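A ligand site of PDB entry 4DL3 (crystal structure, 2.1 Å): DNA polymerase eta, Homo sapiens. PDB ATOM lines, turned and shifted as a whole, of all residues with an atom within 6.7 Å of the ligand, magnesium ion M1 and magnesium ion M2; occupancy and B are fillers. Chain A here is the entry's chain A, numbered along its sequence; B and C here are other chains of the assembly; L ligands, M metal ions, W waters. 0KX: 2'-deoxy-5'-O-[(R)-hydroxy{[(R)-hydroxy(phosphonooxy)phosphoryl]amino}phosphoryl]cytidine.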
ATOM      1  N   ASP A  16       7.678 -10.794  -9.231  1.00  0.00           N
ATOM      2  CA  ASP A  16       8.825 -11.626  -8.946  1.00  0.00           C
ATOM      3  C   ASP A  16       8.490 -13.099  -9.174  1.00  0.00           C
ATOM      4  O   ASP A  16       7.518 -13.613  -8.628  1.00  0.00           O
ATOM      5  CB  ASP A  16       9.271 -11.382  -7.524  1.00  0.00           C
ATOM      6  CG  ASP A  16      10.488 -12.156  -7.169  1.00  0.00           C
ATOM      7  OD1 ASP A  16      10.329 -13.343  -6.812  1.00  0.00           O
ATOM      8  OD2 ASP A  16      11.593 -11.596  -7.268  1.00  0.00           O
ATOM      9  N   MET A  17       9.305 -13.776  -9.982  1.00  0.00           N
ATOM     10  CA  MET A  17       9.068 -15.184 -10.318  1.00  0.00           C
ATOM     11  C   MET A  17       9.246 -16.074  -9.085  1.00  0.00           C
ATOM     12  O   MET A  17      10.118 -15.825  -8.287  1.00  0.00           O
ATOM     13  CB  MET A  17      10.040 -15.637 -11.412  1.00  0.00           C
ATOM     14  CG  MET A  17      10.181 -14.663 -12.565  1.00  0.00           C
ATOM     15  SD  MET A  17       8.608 -14.285 -13.349  1.00  0.00           S
ATOM     16  CE  MET A  17       8.053 -15.926 -13.797  1.00  0.00           C
ATOM     17  N   ASP A  18       8.415 -17.096  -8.945  1.00  0.00           N
ATOM     18  CA  ASP A  18       8.551 -17.987  -7.789  1.00  0.00           C
ATOM     19  C   ASP A  18       9.652 -19.016  -8.032  1.00  0.00           C
ATOM     20  O   ASP A  18       9.644 -19.712  -9.050  1.00  0.00           O
ATOM     21  CB  ASP A  18       7.224 -18.690  -7.510  1.00  0.00           C
ATOM     22  CG  ASP A  18       6.076 -17.727  -7.356  1.00  0.00           C
ATOM     23  OD1 ASP A  18       6.310 -16.572  -6.943  1.00  0.00           O
ATOM     24  OD2 ASP A  18       4.920 -18.117  -7.643  1.00  0.00           O
ATOM     25  N   CYS A  19      10.579 -19.121  -7.090  1.00  0.00           N
ATOM     26  CA  CYS A  19      11.702 -20.056  -7.202  1.00  0.00           C
ATOM     27  C   CYS A  19      12.138 -20.184  -8.661  1.00  0.00           C
ATOM     28  O   CYS A  19      12.069 -21.269  -9.248  1.00  0.00           O
ATOM     29  CB  CYS A  19      11.329 -21.422  -6.616  1.00  0.00           C
ATOM     30  SG  CYS A  19       9.829 -22.152  -7.303  1.00  0.00           S
ATOM     31  N   PHE A  20      12.594 -19.069  -9.226  1.00  0.00           N
ATOM     32  CA  PHE A  20      12.762 -18.925 -10.666  1.00  0.00           C
ATOM     33  C   PHE A  20      13.666 -19.965 -11.347  1.00  0.00           C
ATOM     34  O   PHE A  20      13.257 -20.597 -12.319  1.00  0.00           O
ATOM     35  CB  PHE A  20      13.229 -17.507 -11.012  1.00  0.00           C
ATOM     36  CG  PHE A  20      13.302 -17.243 -12.482  1.00  0.00           C
ATOM     37  CD1 PHE A  20      12.224 -17.534 -13.310  1.00  0.00           C
ATOM     38  CD2 PHE A  20      14.433 -16.688 -13.039  1.00  0.00           C
ATOM     39  CE1 PHE A  20      12.285 -17.284 -14.656  1.00  0.00           C
ATOM     40  CE2 PHE A  20      14.506 -16.426 -14.400  1.00  0.00           C
ATOM     41  CZ  PHE A  20      13.427 -16.729 -15.212  1.00  0.00           C
ATOM     42  N   PHE A  21      14.893 -20.119 -10.854  1.00  0.00           N
ATOM     43  CA  PHE A  21      15.826 -21.067 -11.468  1.00  0.00           C
ATOM     44  C   PHE A  21      15.260 -22.484 -11.435  1.00  0.00           C
ATOM     45  O   PHE A  21      15.450 -23.259 -12.375  1.00  0.00           O
ATOM     46  CB  PHE A  21      17.195 -21.015 -10.806  1.00  0.00           C
ATOM     47  CG  PHE A  21      17.997 -19.794 -11.163  1.00  0.00           C
ATOM     48  CD1 PHE A  21      17.385 -18.685 -11.722  1.00  0.00           C
ATOM     49  CD2 PHE A  21      19.363 -19.761 -10.959  1.00  0.00           C
ATOM     50  CE1 PHE A  21      18.118 -17.555 -12.050  1.00  0.00           C
ATOM     51  CE2 PHE A  21      20.109 -18.647 -11.297  1.00  0.00           C
ATOM     52  CZ  PHE A  21      19.486 -17.537 -11.844  1.00  0.00           C
ATOM     53  N   VAL A  22      14.575 -22.810 -10.354  1.00  0.00           N
ATOM     54  CA  VAL A  22      13.922 -24.113 -10.220  1.00  0.00           C
ATOM     55  C   VAL A  22      12.852 -24.294 -11.289  1.00  0.00           C
ATOM     56  O   VAL A  22      12.755 -25.357 -11.911  1.00  0.00           O
ATOM     57  CB  VAL A  22      13.299 -24.292  -8.832  1.00  0.00           C
ATOM     58  CG1 VAL A  22      12.349 -25.484  -8.821  1.00  0.00           C
ATOM     59  CG2 VAL A  22      14.390 -24.471  -7.774  1.00  0.00           C
ATOM     60  N   GLN A  41      25.123 -25.343  -8.081  1.00  0.00           N
ATOM     61  CA  GLN A  41      26.292 -25.128  -8.916  1.00  0.00           C
ATOM     62  C   GLN A  41      27.534 -25.701  -8.231  1.00  0.00           C
ATOM     63  O   GLN A  41      27.632 -25.698  -7.003  1.00  0.00           O
ATOM     64  CB  GLN A  41      26.471 -23.640  -9.242  1.00  0.00           C
ATOM     65  CG  GLN A  41      26.406 -22.726  -8.022  1.00  0.00           C
ATOM     66  CD  GLN A  41      26.599 -21.258  -8.385  1.00  0.00           C
ATOM     67  OE1 GLN A  41      26.327 -20.850  -9.513  1.00  0.00           O
ATOM     68  NE2 GLN A  41      27.072 -20.483  -7.430  1.00  0.00           N
ATOM     69  N   ILE A  51      21.306 -22.649  -4.929  1.00  0.00           N
ATOM     70  CA  ILE A  51      21.026 -21.256  -5.239  1.00  0.00           C
ATOM     71  C   ILE A  51      19.534 -20.989  -5.470  1.00  0.00           C
ATOM     72  O   ILE A  51      19.105 -19.837  -5.468  1.00  0.00           O
ATOM     73  CB  ILE A  51      21.862 -20.742  -6.435  1.00  0.00           C
ATOM     74  CG1 ILE A  51      21.355 -21.342  -7.748  1.00  0.00           C
ATOM     75  CG2 ILE A  51      23.329 -21.056  -6.228  1.00  0.00           C
ATOM     76  CD1 ILE A  51      22.083 -20.823  -8.971  1.00  0.00           C
ATOM     77  N   ALA A  52      18.759 -22.051  -5.662  1.00  0.00           N
ATOM     78  CA  ALA A  52      17.318 -21.928  -5.820  1.00  0.00           C
ATOM     79  C   ALA A  52      16.591 -23.127  -5.221  1.00  0.00           C
ATOM     80  O   ALA A  52      17.070 -24.259  -5.328  1.00  0.00           O
ATOM     81  CB  ALA A  52      16.952 -21.751  -7.281  1.00  0.00           C
ATOM     82  N   VAL A  53      15.438 -22.890  -4.602  1.00  0.00           N
ATOM     83  CA  VAL A  53      14.723 -23.955  -3.893  1.00  0.00           C
ATOM     84  C   VAL A  53      13.222 -23.951  -4.190  1.00  0.00           C
ATOM     85  O   VAL A  53      12.554 -22.926  -4.035  1.00  0.00           O
ATOM     86  CB  VAL A  53      14.925 -23.840  -2.369  1.00  0.00           C
ATOM     87  CG1 VAL A  53      14.256 -25.005  -1.668  1.00  0.00           C
ATOM     88  CG2 VAL A  53      16.407 -23.780  -2.028  1.00  0.00           C
ATOM     89  N   TYR A  55       9.253 -24.805  -3.573  1.00  0.00           N
ATOM     90  CA  TYR A  55       8.467 -24.646  -2.360  1.00  0.00           C
ATOM     91  C   TYR A  55       8.208 -25.957  -1.640  1.00  0.00           C
ATOM     92  O   TYR A  55       8.076 -25.993  -0.416  1.00  0.00           O
ATOM     93  CB  TYR A  55       7.173 -23.880  -2.650  1.00  0.00           C
ATOM     94  CG  TYR A  55       7.413 -22.399  -2.780  1.00  0.00           C
ATOM     95  CD1 TYR A  55       7.835 -21.851  -3.976  1.00  0.00           C
ATOM     96  CD2 TYR A  55       7.244 -21.555  -1.690  1.00  0.00           C
ATOM     97  CE1 TYR A  55       8.070 -20.491  -4.094  1.00  0.00           C
ATOM     98  CE2 TYR A  55       7.479 -20.206  -1.792  1.00  0.00           C
ATOM     99  CZ  TYR A  55       7.892 -19.675  -3.001  1.00  0.00           C
ATOM    100  OH  TYR A  55       8.127 -18.327  -3.102  1.00  0.00           O
ATOM    101  N   ARG A  58      11.313 -26.327   0.314  1.00  0.00           N
ATOM    102  CA  ARG A  58      11.388 -25.376   1.420  1.00  0.00           C
ATOM    103  C   ARG A  58      10.620 -25.884   2.637  1.00  0.00           C
ATOM    104  O   ARG A  58      10.916 -25.508   3.776  1.00  0.00           O
ATOM    105  CB  ARG A  58      10.860 -24.000   0.985  1.00  0.00           C
ATOM    106  CG  ARG A  58      11.627 -23.397  -0.175  1.00  0.00           C
ATOM    107  CD  ARG A  58      11.118 -21.997  -0.519  1.00  0.00           C
ATOM    108  NE  ARG A  58      11.671 -21.520  -1.783  1.00  0.00           N
ATOM    109  CZ  ARG A  58      11.487 -20.294  -2.257  1.00  0.00           C
ATOM    110  NH1 ARG A  58      10.763 -19.410  -1.566  1.00  0.00           N
ATOM    111  NH2 ARG A  58      12.018 -19.938  -3.424  1.00  0.00           N
ATOM    112  N   ARG A  64      18.487 -21.553   0.425  1.00  0.00           N
ATOM    113  CA  ARG A  64      19.526 -21.086  -0.460  1.00  0.00           C
ATOM    114  C   ARG A  64      20.817 -20.956   0.339  1.00  0.00           C
ATOM    115  O   ARG A  64      20.789 -20.609   1.512  1.00  0.00           O
ATOM    116  CB  ARG A  64      19.137 -19.732  -1.063  1.00  0.00           C
ATOM    117  CG  ARG A  64      20.265 -19.017  -1.777  1.00  0.00           C
ATOM    118  CD  ARG A  64      19.781 -17.763  -2.483  1.00  0.00           C
ATOM    119  NE  ARG A  64      19.218 -16.797  -1.550  1.00  0.00           N
ATOM    120  CZ  ARG A  64      17.933 -16.522  -1.442  1.00  0.00           C
ATOM    121  NH1 ARG A  64      17.510 -15.629  -0.554  1.00  0.00           N
ATOM    122  NH2 ARG A  64      17.050 -17.133  -2.218  1.00  0.00           N
ATOM    123  N   LEU A  92      25.256 -18.907 -16.553  1.00  0.00           N
ATOM    124  CA  LEU A  92      23.882 -18.587 -16.195  1.00  0.00           C
ATOM    125  C   LEU A  92      23.006 -18.235 -17.388  1.00  0.00           C
ATOM    126  O   LEU A  92      21.949 -17.634 -17.228  1.00  0.00           O
ATOM    127  CB  LEU A  92      23.855 -17.434 -15.183  1.00  0.00           C
ATOM    128  CG  LEU A  92      24.621 -17.649 -13.874  1.00  0.00           C
ATOM    129  CD1 LEU A  92      24.346 -16.519 -12.893  1.00  0.00           C
ATOM    130  CD2 LEU A  92      24.243 -18.989 -13.257  1.00  0.00           C
ATOM    131  N   SER A 116      15.999  -7.342 -11.148  1.00  0.00           N
ATOM    132  CA  SER A 116      16.853  -8.519 -11.055  1.00  0.00           C
ATOM    133  C   SER A 116      16.571  -9.458 -12.215  1.00  0.00           C
ATOM    134  O   SER A 116      15.756  -9.164 -13.089  1.00  0.00           O
ATOM    135  CB  SER A 116      16.620  -9.245  -9.729  1.00  0.00           C
ATOM    136  OG  SER A 116      15.454 -10.042  -9.792  1.00  0.00           O
ATOM    137  N   ILE A 117      17.251 -10.607 -12.211  1.00  0.00           N
ATOM    138  CA  ILE A 117      17.061 -11.593 -13.253  1.00  0.00           C
ATOM    139  C   ILE A 117      15.630 -12.123 -13.237  1.00  0.00           C
ATOM    140  O   ILE A 117      15.059 -12.443 -14.279  1.00  0.00           O
ATOM    141  CB  ILE A 117      18.061 -12.765 -13.123  1.00  0.00           C
ATOM    142  CG1 ILE A 117      18.108 -13.583 -14.411  1.00  0.00           C
ATOM    143  CG2 ILE A 117      17.719 -13.639 -11.922  1.00  0.00           C
ATOM    144  CD1 ILE A 117      19.176 -14.658 -14.404  1.00  0.00           C
ATOM    145  N   ASP A 118      15.032 -12.213 -12.056  1.00  0.00           N
ATOM    146  CA  ASP A 118      13.719 -12.818 -11.965  1.00  0.00           C
ATOM    147  C   ASP A 118      12.613 -11.825 -11.551  1.00  0.00           C
ATOM    148  O   ASP A 118      11.490 -12.243 -11.253  1.00  0.00           O
ATOM    149  CB  ASP A 118      13.746 -13.972 -10.980  1.00  0.00           C
ATOM    150  CG  ASP A 118      13.236 -13.567  -9.647  1.00  0.00           C
ATOM    151  OD1 ASP A 118      12.268 -14.187  -9.176  1.00  0.00           O
ATOM    152  OD2 ASP A 118      13.779 -12.591  -9.098  1.00  0.00           O
ATOM    153  N   GLU A 119      12.920 -10.539 -11.533  1.00  0.00           N
ATOM    154  CA  GLU A 119      11.891  -9.553 -11.182  1.00  0.00           C
ATOM    155  C   GLU A 119      12.073  -8.196 -11.860  1.00  0.00           C
ATOM    156  O   GLU A 119      13.176  -7.812 -12.234  1.00  0.00           O
ATOM    157  CB  GLU A 119      11.809  -9.380  -9.669  1.00  0.00           C
ATOM    158  CG  GLU A 119      12.833  -8.409  -9.096  1.00  0.00           C
ATOM    159  CD  GLU A 119      13.222  -8.756  -7.669  1.00  0.00           C
ATOM    160  OE1 GLU A 119      12.893  -7.983  -6.751  1.00  0.00           O
ATOM    161  OE2 GLU A 119      13.858  -9.804  -7.485  1.00  0.00           O
ATOM    162  N   SER A 216       4.708 -14.086  -8.544  1.00  0.00           N
ATOM    163  CA  SER A 216       3.922 -13.337  -7.571  1.00  0.00           C
ATOM    164  C   SER A 216       4.159 -11.854  -7.774  1.00  0.00           C
ATOM    165  O   SER A 216       5.163 -11.462  -8.369  1.00  0.00           O
ATOM    166  CB  SER A 216       4.296 -13.757  -6.149  1.00  0.00           C
ATOM    167  OG  SER A 216       4.021 -15.131  -5.933  1.00  0.00           O
ATOM    168  N   LYS A 227       7.329  -4.238  -3.541  1.00  0.00           N
ATOM    169  CA  LYS A 227       8.263  -5.334  -3.286  1.00  0.00           C
ATOM    170  C   LYS A 227       7.904  -6.080  -2.007  1.00  0.00           C
ATOM    171  O   LYS A 227       7.854  -7.315  -1.998  1.00  0.00           O
ATOM    172  CB  LYS A 227       9.692  -4.800  -3.187  1.00  0.00           C
ATOM    173  CG  LYS A 227      10.719  -5.819  -2.712  1.00  0.00           C
ATOM    174  CD  LYS A 227      10.802  -7.001  -3.655  1.00  0.00           C
ATOM    175  CE  LYS A 227      12.017  -7.860  -3.337  1.00  0.00           C
ATOM    176  NZ  LYS A 227      12.159  -9.010  -4.278  1.00  0.00           N
ATOM    177  N   LYS A 234       3.462 -15.073  -1.535  1.00  0.00           N
ATOM    178  CA  LYS A 234       4.128 -16.050  -2.382  1.00  0.00           C
ATOM    179  C   LYS A 234       3.824 -17.454  -1.869  1.00  0.00           C
ATOM    180  O   LYS A 234       3.643 -17.645  -0.661  1.00  0.00           O
ATOM    181  CB  LYS A 234       5.645 -15.824  -2.389  1.00  0.00           C
ATOM    182  CG  LYS A 234       6.159 -15.002  -3.555  1.00  0.00           C
ATOM    183  CD  LYS A 234       7.681 -14.908  -3.532  1.00  0.00           C
ATOM    184  CE  LYS A 234       8.223 -14.155  -4.734  1.00  0.00           C
ATOM    185  NZ  LYS A 234       8.134 -14.952  -5.990  1.00  0.00           N
ATOM    186  N   PRO A 235       3.772 -18.448  -2.771  1.00  0.00           N
ATOM    187  CA  PRO A 235       3.968 -18.287  -4.210  1.00  0.00           C
ATOM    188  C   PRO A 235       2.658 -18.260  -5.008  1.00  0.00           C
ATOM    189  O   PRO A 235       1.594 -18.557  -4.471  1.00  0.00           O
ATOM    190  CB  PRO A 235       4.752 -19.538  -4.581  1.00  0.00           C
ATOM    191  CG  PRO A 235       4.195 -20.581  -3.650  1.00  0.00           C
ATOM    192  CD  PRO A 235       3.812 -19.864  -2.368  1.00  0.00           C
ATOM    193  P    DC B   9      15.909  -7.454  -3.528  1.00  0.00           P
ATOM    194  OP1  DC B   9      14.878  -6.721  -4.295  1.00  0.00           O
ATOM    195  OP2  DC B   9      15.659  -7.844  -2.122  1.00  0.00           O
ATOM    196  O5'  DC B   9      16.319  -8.759  -4.343  1.00  0.00           O
ATOM    197  C5'  DC B   9      16.577  -8.690  -5.745  1.00  0.00           C
ATOM    198  C4'  DC B   9      17.233  -9.951  -6.230  1.00  0.00           C
ATOM    199  O4'  DC B   9      18.598 -10.024  -5.757  1.00  0.00           O
ATOM    200  C3'  DC B   9      16.568 -11.258  -5.779  1.00  0.00           C
ATOM    201  O3'  DC B   9      15.984 -11.897  -6.914  1.00  0.00           O
ATOM    202  C2'  DC B   9      17.717 -12.086  -5.221  1.00  0.00           C
ATOM    203  C1'  DC B   9      18.949 -11.387  -5.754  1.00  0.00           C
ATOM    204  N1   DC B   9      20.175 -11.534  -4.960  1.00  0.00           N
ATOM    205  C2   DC B   9      21.333 -11.956  -5.614  1.00  0.00           C
ATOM    206  O2   DC B   9      21.288 -12.184  -6.828  1.00  0.00           O
ATOM    207  N3   DC B   9      22.477 -12.091  -4.903  1.00  0.00           N
ATOM    208  C4   DC B   9      22.481 -11.821  -3.599  1.00  0.00           C
ATOM    209  N4   DC B   9      23.630 -11.971  -2.935  1.00  0.00           N
ATOM    210  C5   DC B   9      21.309 -11.387  -2.913  1.00  0.00           C
ATOM    211  C6   DC B   9      20.196 -11.258  -3.627  1.00  0.00           C
ATOM    212  P    DG C   4      31.450 -18.819  -1.892  1.00  0.00           P
ATOM    213  OP1  DG C   4      31.924 -20.152  -1.441  1.00  0.00           O
ATOM    214  OP2  DG C   4      32.394 -17.680  -1.917  1.00  0.00           O
ATOM    215  O5'  DG C   4      30.819 -18.959  -3.337  1.00  0.00           O
ATOM    216  C5'  DG C   4      30.915 -20.199  -4.075  1.00  0.00           C
ATOM    217  C4'  DG C   4      30.451 -19.976  -5.496  1.00  0.00           C
ATOM    218  O4'  DG C   4      29.082 -19.490  -5.475  1.00  0.00           O
ATOM    219  C3'  DG C   4      31.244 -18.933  -6.264  1.00  0.00           C
ATOM    220  O3'  DG C   4      31.284 -19.306  -7.640  1.00  0.00           O
ATOM    221  C2'  DG C   4      30.443 -17.656  -6.036  1.00  0.00           C
ATOM    222  C1'  DG C   4      29.019 -18.180  -5.992  1.00  0.00           C
ATOM    223  N9   DG C   4      28.105 -17.416  -5.152  1.00  0.00           N
ATOM    224  C8   DG C   4      28.401 -16.774  -3.970  1.00  0.00           C
ATOM    225  N7   DG C   4      27.377 -16.174  -3.439  1.00  0.00           N
ATOM    226  C5   DG C   4      26.333 -16.442  -4.311  1.00  0.00           C
ATOM    227  C6   DG C   4      24.966 -16.051  -4.259  1.00  0.00           C
ATOM    228  O6   DG C   4      24.387 -15.383  -3.395  1.00  0.00           O
ATOM    229  N1   DG C   4      24.259 -16.537  -5.353  1.00  0.00           N
ATOM    230  C2   DG C   4      24.787 -17.289  -6.368  1.00  0.00           C
ATOM    231  N2   DG C   4      23.940 -17.665  -7.330  1.00  0.00           N
ATOM    232  N3   DG C   4      26.054 -17.658  -6.434  1.00  0.00           N
ATOM    233  C4   DG C   4      26.766 -17.207  -5.377  1.00  0.00           C
ATOM    234  P    DG C   5      31.815 -18.326  -8.766  1.00  0.00           P
ATOM    235  OP1  DG C   5      32.403 -19.177  -9.822  1.00  0.00           O
ATOM    236  OP2  DG C   5      32.653 -17.329  -8.072  1.00  0.00           O
ATOM    237  O5'  DG C   5      30.552 -17.560  -9.363  1.00  0.00           O
ATOM    238  C5'  DG C   5      29.571 -18.270 -10.104  1.00  0.00           C
ATOM    239  C4'  DG C   5      28.539 -17.334 -10.689  1.00  0.00           C
ATOM    240  O4'  DG C   5      27.705 -16.773  -9.633  1.00  0.00           O
ATOM    241  C3'  DG C   5      29.127 -16.134 -11.419  1.00  0.00           C
ATOM    242  O3'  DG C   5      28.289 -15.735 -12.514  1.00  0.00           O
ATOM    243  C2'  DG C   5      29.145 -15.110 -10.287  1.00  0.00           C
ATOM    244  C1'  DG C   5      27.764 -15.372  -9.720  1.00  0.00           C
ATOM    245  N9   DG C   5      27.556 -14.784  -8.397  1.00  0.00           N
ATOM    246  C8   DG C   5      28.506 -14.605  -7.435  1.00  0.00           C
ATOM    247  N7   DG C   5      28.042 -14.054  -6.351  1.00  0.00           N
ATOM    248  C5   DG C   5      26.699 -13.852  -6.620  1.00  0.00           C
ATOM    249  C6   DG C   5      25.679 -13.285  -5.816  1.00  0.00           C
ATOM    250  O6   DG C   5      25.768 -12.835  -4.662  1.00  0.00           O
ATOM    251  N1   DG C   5      24.456 -13.273  -6.472  1.00  0.00           N
ATOM    252  C2   DG C   5      24.230 -13.749  -7.753  1.00  0.00           C
ATOM    253  N2   DG C   5      22.983 -13.655  -8.216  1.00  0.00           N
ATOM    254  N3   DG C   5      25.183 -14.283  -8.511  1.00  0.00           N
ATOM    255  C4   DG C   5      26.378 -14.293  -7.880  1.00  0.00           C
HETATM  256  PG  0KX L   1      11.085 -16.735  -4.593  1.00  0.00           P
HETATM  257  O1G 0KX L   1      11.150 -16.592  -3.117  1.00  0.00           O
HETATM  258  O2G 0KX L   1      11.165 -15.419  -5.233  1.00  0.00           O
HETATM  259  O3G 0KX L   1       9.826 -17.332  -4.937  1.00  0.00           O
HETATM  260  PB  0KX L   1      13.439 -17.258  -5.963  1.00  0.00           P
HETATM  261  O1B 0KX L   1      14.197 -18.515  -6.278  1.00  0.00           O
HETATM  262  O2B 0KX L   1      13.025 -16.643  -7.198  1.00  0.00           O
HETATM  263  O3B 0KX L   1      12.217 -17.683  -5.084  1.00  0.00           O
HETATM  264  PA  0KX L   1      14.746 -14.746  -5.682  1.00  0.00           P
HETATM  265  O1A 0KX L   1      13.415 -14.161  -6.401  1.00  0.00           O
HETATM  266  O2A 0KX L   1      15.168 -13.802  -4.522  1.00  0.00           O
HETATM  267  N3A 0KX L   1      14.384 -16.252  -5.036  1.00  0.00           N
HETATM  268  O5' 0KX L   1      15.880 -14.870  -6.776  1.00  0.00           O
HETATM  269  C5' 0KX L   1      15.602 -15.294  -8.071  1.00  0.00           C
HETATM  270  C4' 0KX L   1      16.597 -16.156  -8.656  1.00  0.00           C
HETATM  271  O4' 0KX L   1      17.885 -15.489  -8.630  1.00  0.00           O
HETATM  272  C3' 0KX L   1      16.735 -17.361  -7.837  1.00  0.00           C
HETATM  273  O3' 0KX L   1      16.008 -18.332  -8.357  1.00  0.00           O
HETATM  274  C2' 0KX L   1      18.165 -17.688  -7.950  1.00  0.00           C
HETATM  275  C1' 0KX L   1      18.844 -16.387  -8.146  1.00  0.00           C
HETATM  276  N1  0KX L   1      19.516 -16.038  -6.918  1.00  0.00           N
HETATM  277  C2  0KX L   1      20.816 -16.340  -6.761  1.00  0.00           C
HETATM  278  N3  0KX L   1      21.482 -16.020  -5.666  1.00  0.00           N
HETATM  279  C4  0KX L   1      20.859 -15.419  -4.629  1.00  0.00           C
HETATM  280  C5  0KX L   1      19.515 -15.107  -4.757  1.00  0.00           C
HETATM  281  C6  0KX L   1      18.848 -15.427  -5.939  1.00  0.00           C
HETATM  282  O2  0KX L   1      21.386 -16.838  -7.640  1.00  0.00           O
HETATM  283  N4  0KX L   1      21.551 -15.131  -3.469  1.00  0.00           N
HETATM  284 MG    MG M   1      11.705 -15.047  -7.202  1.00  0.00          MG
HETATM  285 MG    MG M   2      13.855 -12.029  -6.890  1.00  0.00          MG
HETATM  286  O   HOH W   1      22.689 -16.664 -10.371  1.00  0.00           O
HETATM  287  O   HOH W   2      17.619 -12.628  -8.624  1.00  0.00           O
HETATM  288  O   HOH W   3      14.596 -20.334  -4.307  1.00  0.00           O
HETATM  289  O   HOH W   4      13.510 -16.780  -2.162  1.00  0.00           O
HETATM  290  O   HOH W   5      20.037 -14.158  -1.294  1.00  0.00           O
HETATM  291  O   HOH W   6      11.457 -12.931  -4.167  1.00  0.00           O
HETATM  292  O   HOH W   7      13.545 -11.509  -4.919  1.00  0.00           O
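Water W7 is bound to magnesium ion M2, at 2.1 Å. Magnesium ion M2 is bound by O3' of DC 9 of chain B (2.1 Å). Magnesium ion M2 is bound by O1A of the ligand (2.2 Å). Magnesium ion M2 is bound by OD2 of Asp 118, at 2.3 Å. Magnesium ion M2 is bound by the side-chain carboxylate (OE2) of Glu 119, at 2.3 Å. Magnesium ion M2 is bound by OD2 of Asp 16, at 2.3 Å. Magnesium ion M2 has six donor atoms within binding distance.
N4 of the ligand lies close to N3 of DC 9 of chain B (3.5 Å). An oxygen (O3G) of the ligand lies within hydrogen-bond range of the side-chain hydroxyl (OH) of Tyr 55, 2.7 Å away. O6 of DG 4 of chain C lies within hydrogen-bond range of a nitrogen (N4) of the ligand, at 2.8 Å. NH1 of Arg 58 is in salt-bridge range of O1G of the ligand, 3.2 Å away. The backbone NH (N) of Cys 19 sits at hydrogen-bond distance from an oxygen (O3G) of the ligand, at 2.9 Å. The side-chain amino group (NZ) of Lys 234 is in salt-bridge range of an oxygen (O3G) of the ligand, 3.1 Å away. N of Phe 20 sits at hydrogen-bond distance from O1B of the ligand, 3.4 Å away. N of Phe 21 sits at hydrogen-bond distance from O3' of the ligand, at 3.3 Å.
Magnesium ion M1 is bound by an oxygen (O2B) of the ligand (2.1 Å), the backbone carbonyl oxygen (O) of Met 17 (2.1 Å), an oxygen (O2G) of the ligand (2.1 Å), an oxygen (O1A) of the ligand (2.1 Å), the side-chain carboxylate (OD1) of Asp 16 (2.2 Å) and the side-chain carboxylate (OD1) of Asp 118 (2.2 Å).
NE of Arg 64 lies close to N4 of the ligand. CA of Asp 18 touches O3G of the ligand (3.2 Å). Ile 51 touches the ligand. Ala 52 touches the ligand. Ile 117 touches the ligand. DG 5 of chain C touches the ligand. 17 residues have an atom within 4 Å of the ligand: Asp 16, Met 17, Asp 18, Cys 19, Phe 20, Phe 21, Ile 51, Ala 52, Tyr 55, Arg 58, Arg 64, Ile 117, Asp 118, Lys 234, DC 9 of chain B, DG 4 of chain C and DG 5 of chain C. The nearest printed residue that does not touch the ligand is Glu 119 (4.5 Å).
N2 of DG 5 of chain C lies close to O2 of DC 9 of chain B (2.6 Å). The side-chain hydroxyl (OG) of Ser 116 sits close to O3' of DC 9 of chain B (3.5 Å). The side-chain amino group of Lys 227 lies close to the side-chain carboxylate of Asp 16 (3.99 Å). N of Asp 16 sits at hydrogen-bond distance from O of Ser 216. N of Glu 119 lies within hydrogen-bond range of OG of Ser 116 (3.1 Å). The side-chain carboxylate (OE1) of Glu 119 lies within salt-bridge range of the side-chain amino group (NZ) of Lys 227 (2.8 Å). O4' of DG 4 of chain C lies within hydrogen-bond range of NE2 of Gln 41. The side-chain amino group (NZ) of Lys 234 lies within salt-bridge range of the side-chain carboxylate (OD1) of Asp 18 (2.6 Å).
Water W7 bridges an oxygen (O2A) of the ligand and the side-chain amino group of Lys 227. Water W3 lies within hydrogen-bond range of N of Val 53, O1B of the ligand and NH2 of Arg 58. Water W5 bridges NE of Arg 64 (2.8 Å) and N4 of the ligand (2.8 Å). Water W1 lies within hydrogen-bond range of O2 of the ligand (3.0 Å) and N2 of DG 4 of chain C (3.4 Å).
Residues that only touch magnesium ion M2: Ser 116 (3.9 Å). Of the 26 residues printed, 5 come within 4 Å of magnesium ion M2. The nearest printed residue that does not touch magnesium ion M2 is Lys 227 (4.3 Å).
Lys 234 touches magnesium ion M1. Within 4 Å of magnesium ion M1: Asp 16, Met 17, Asp 118 and Lys 234.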
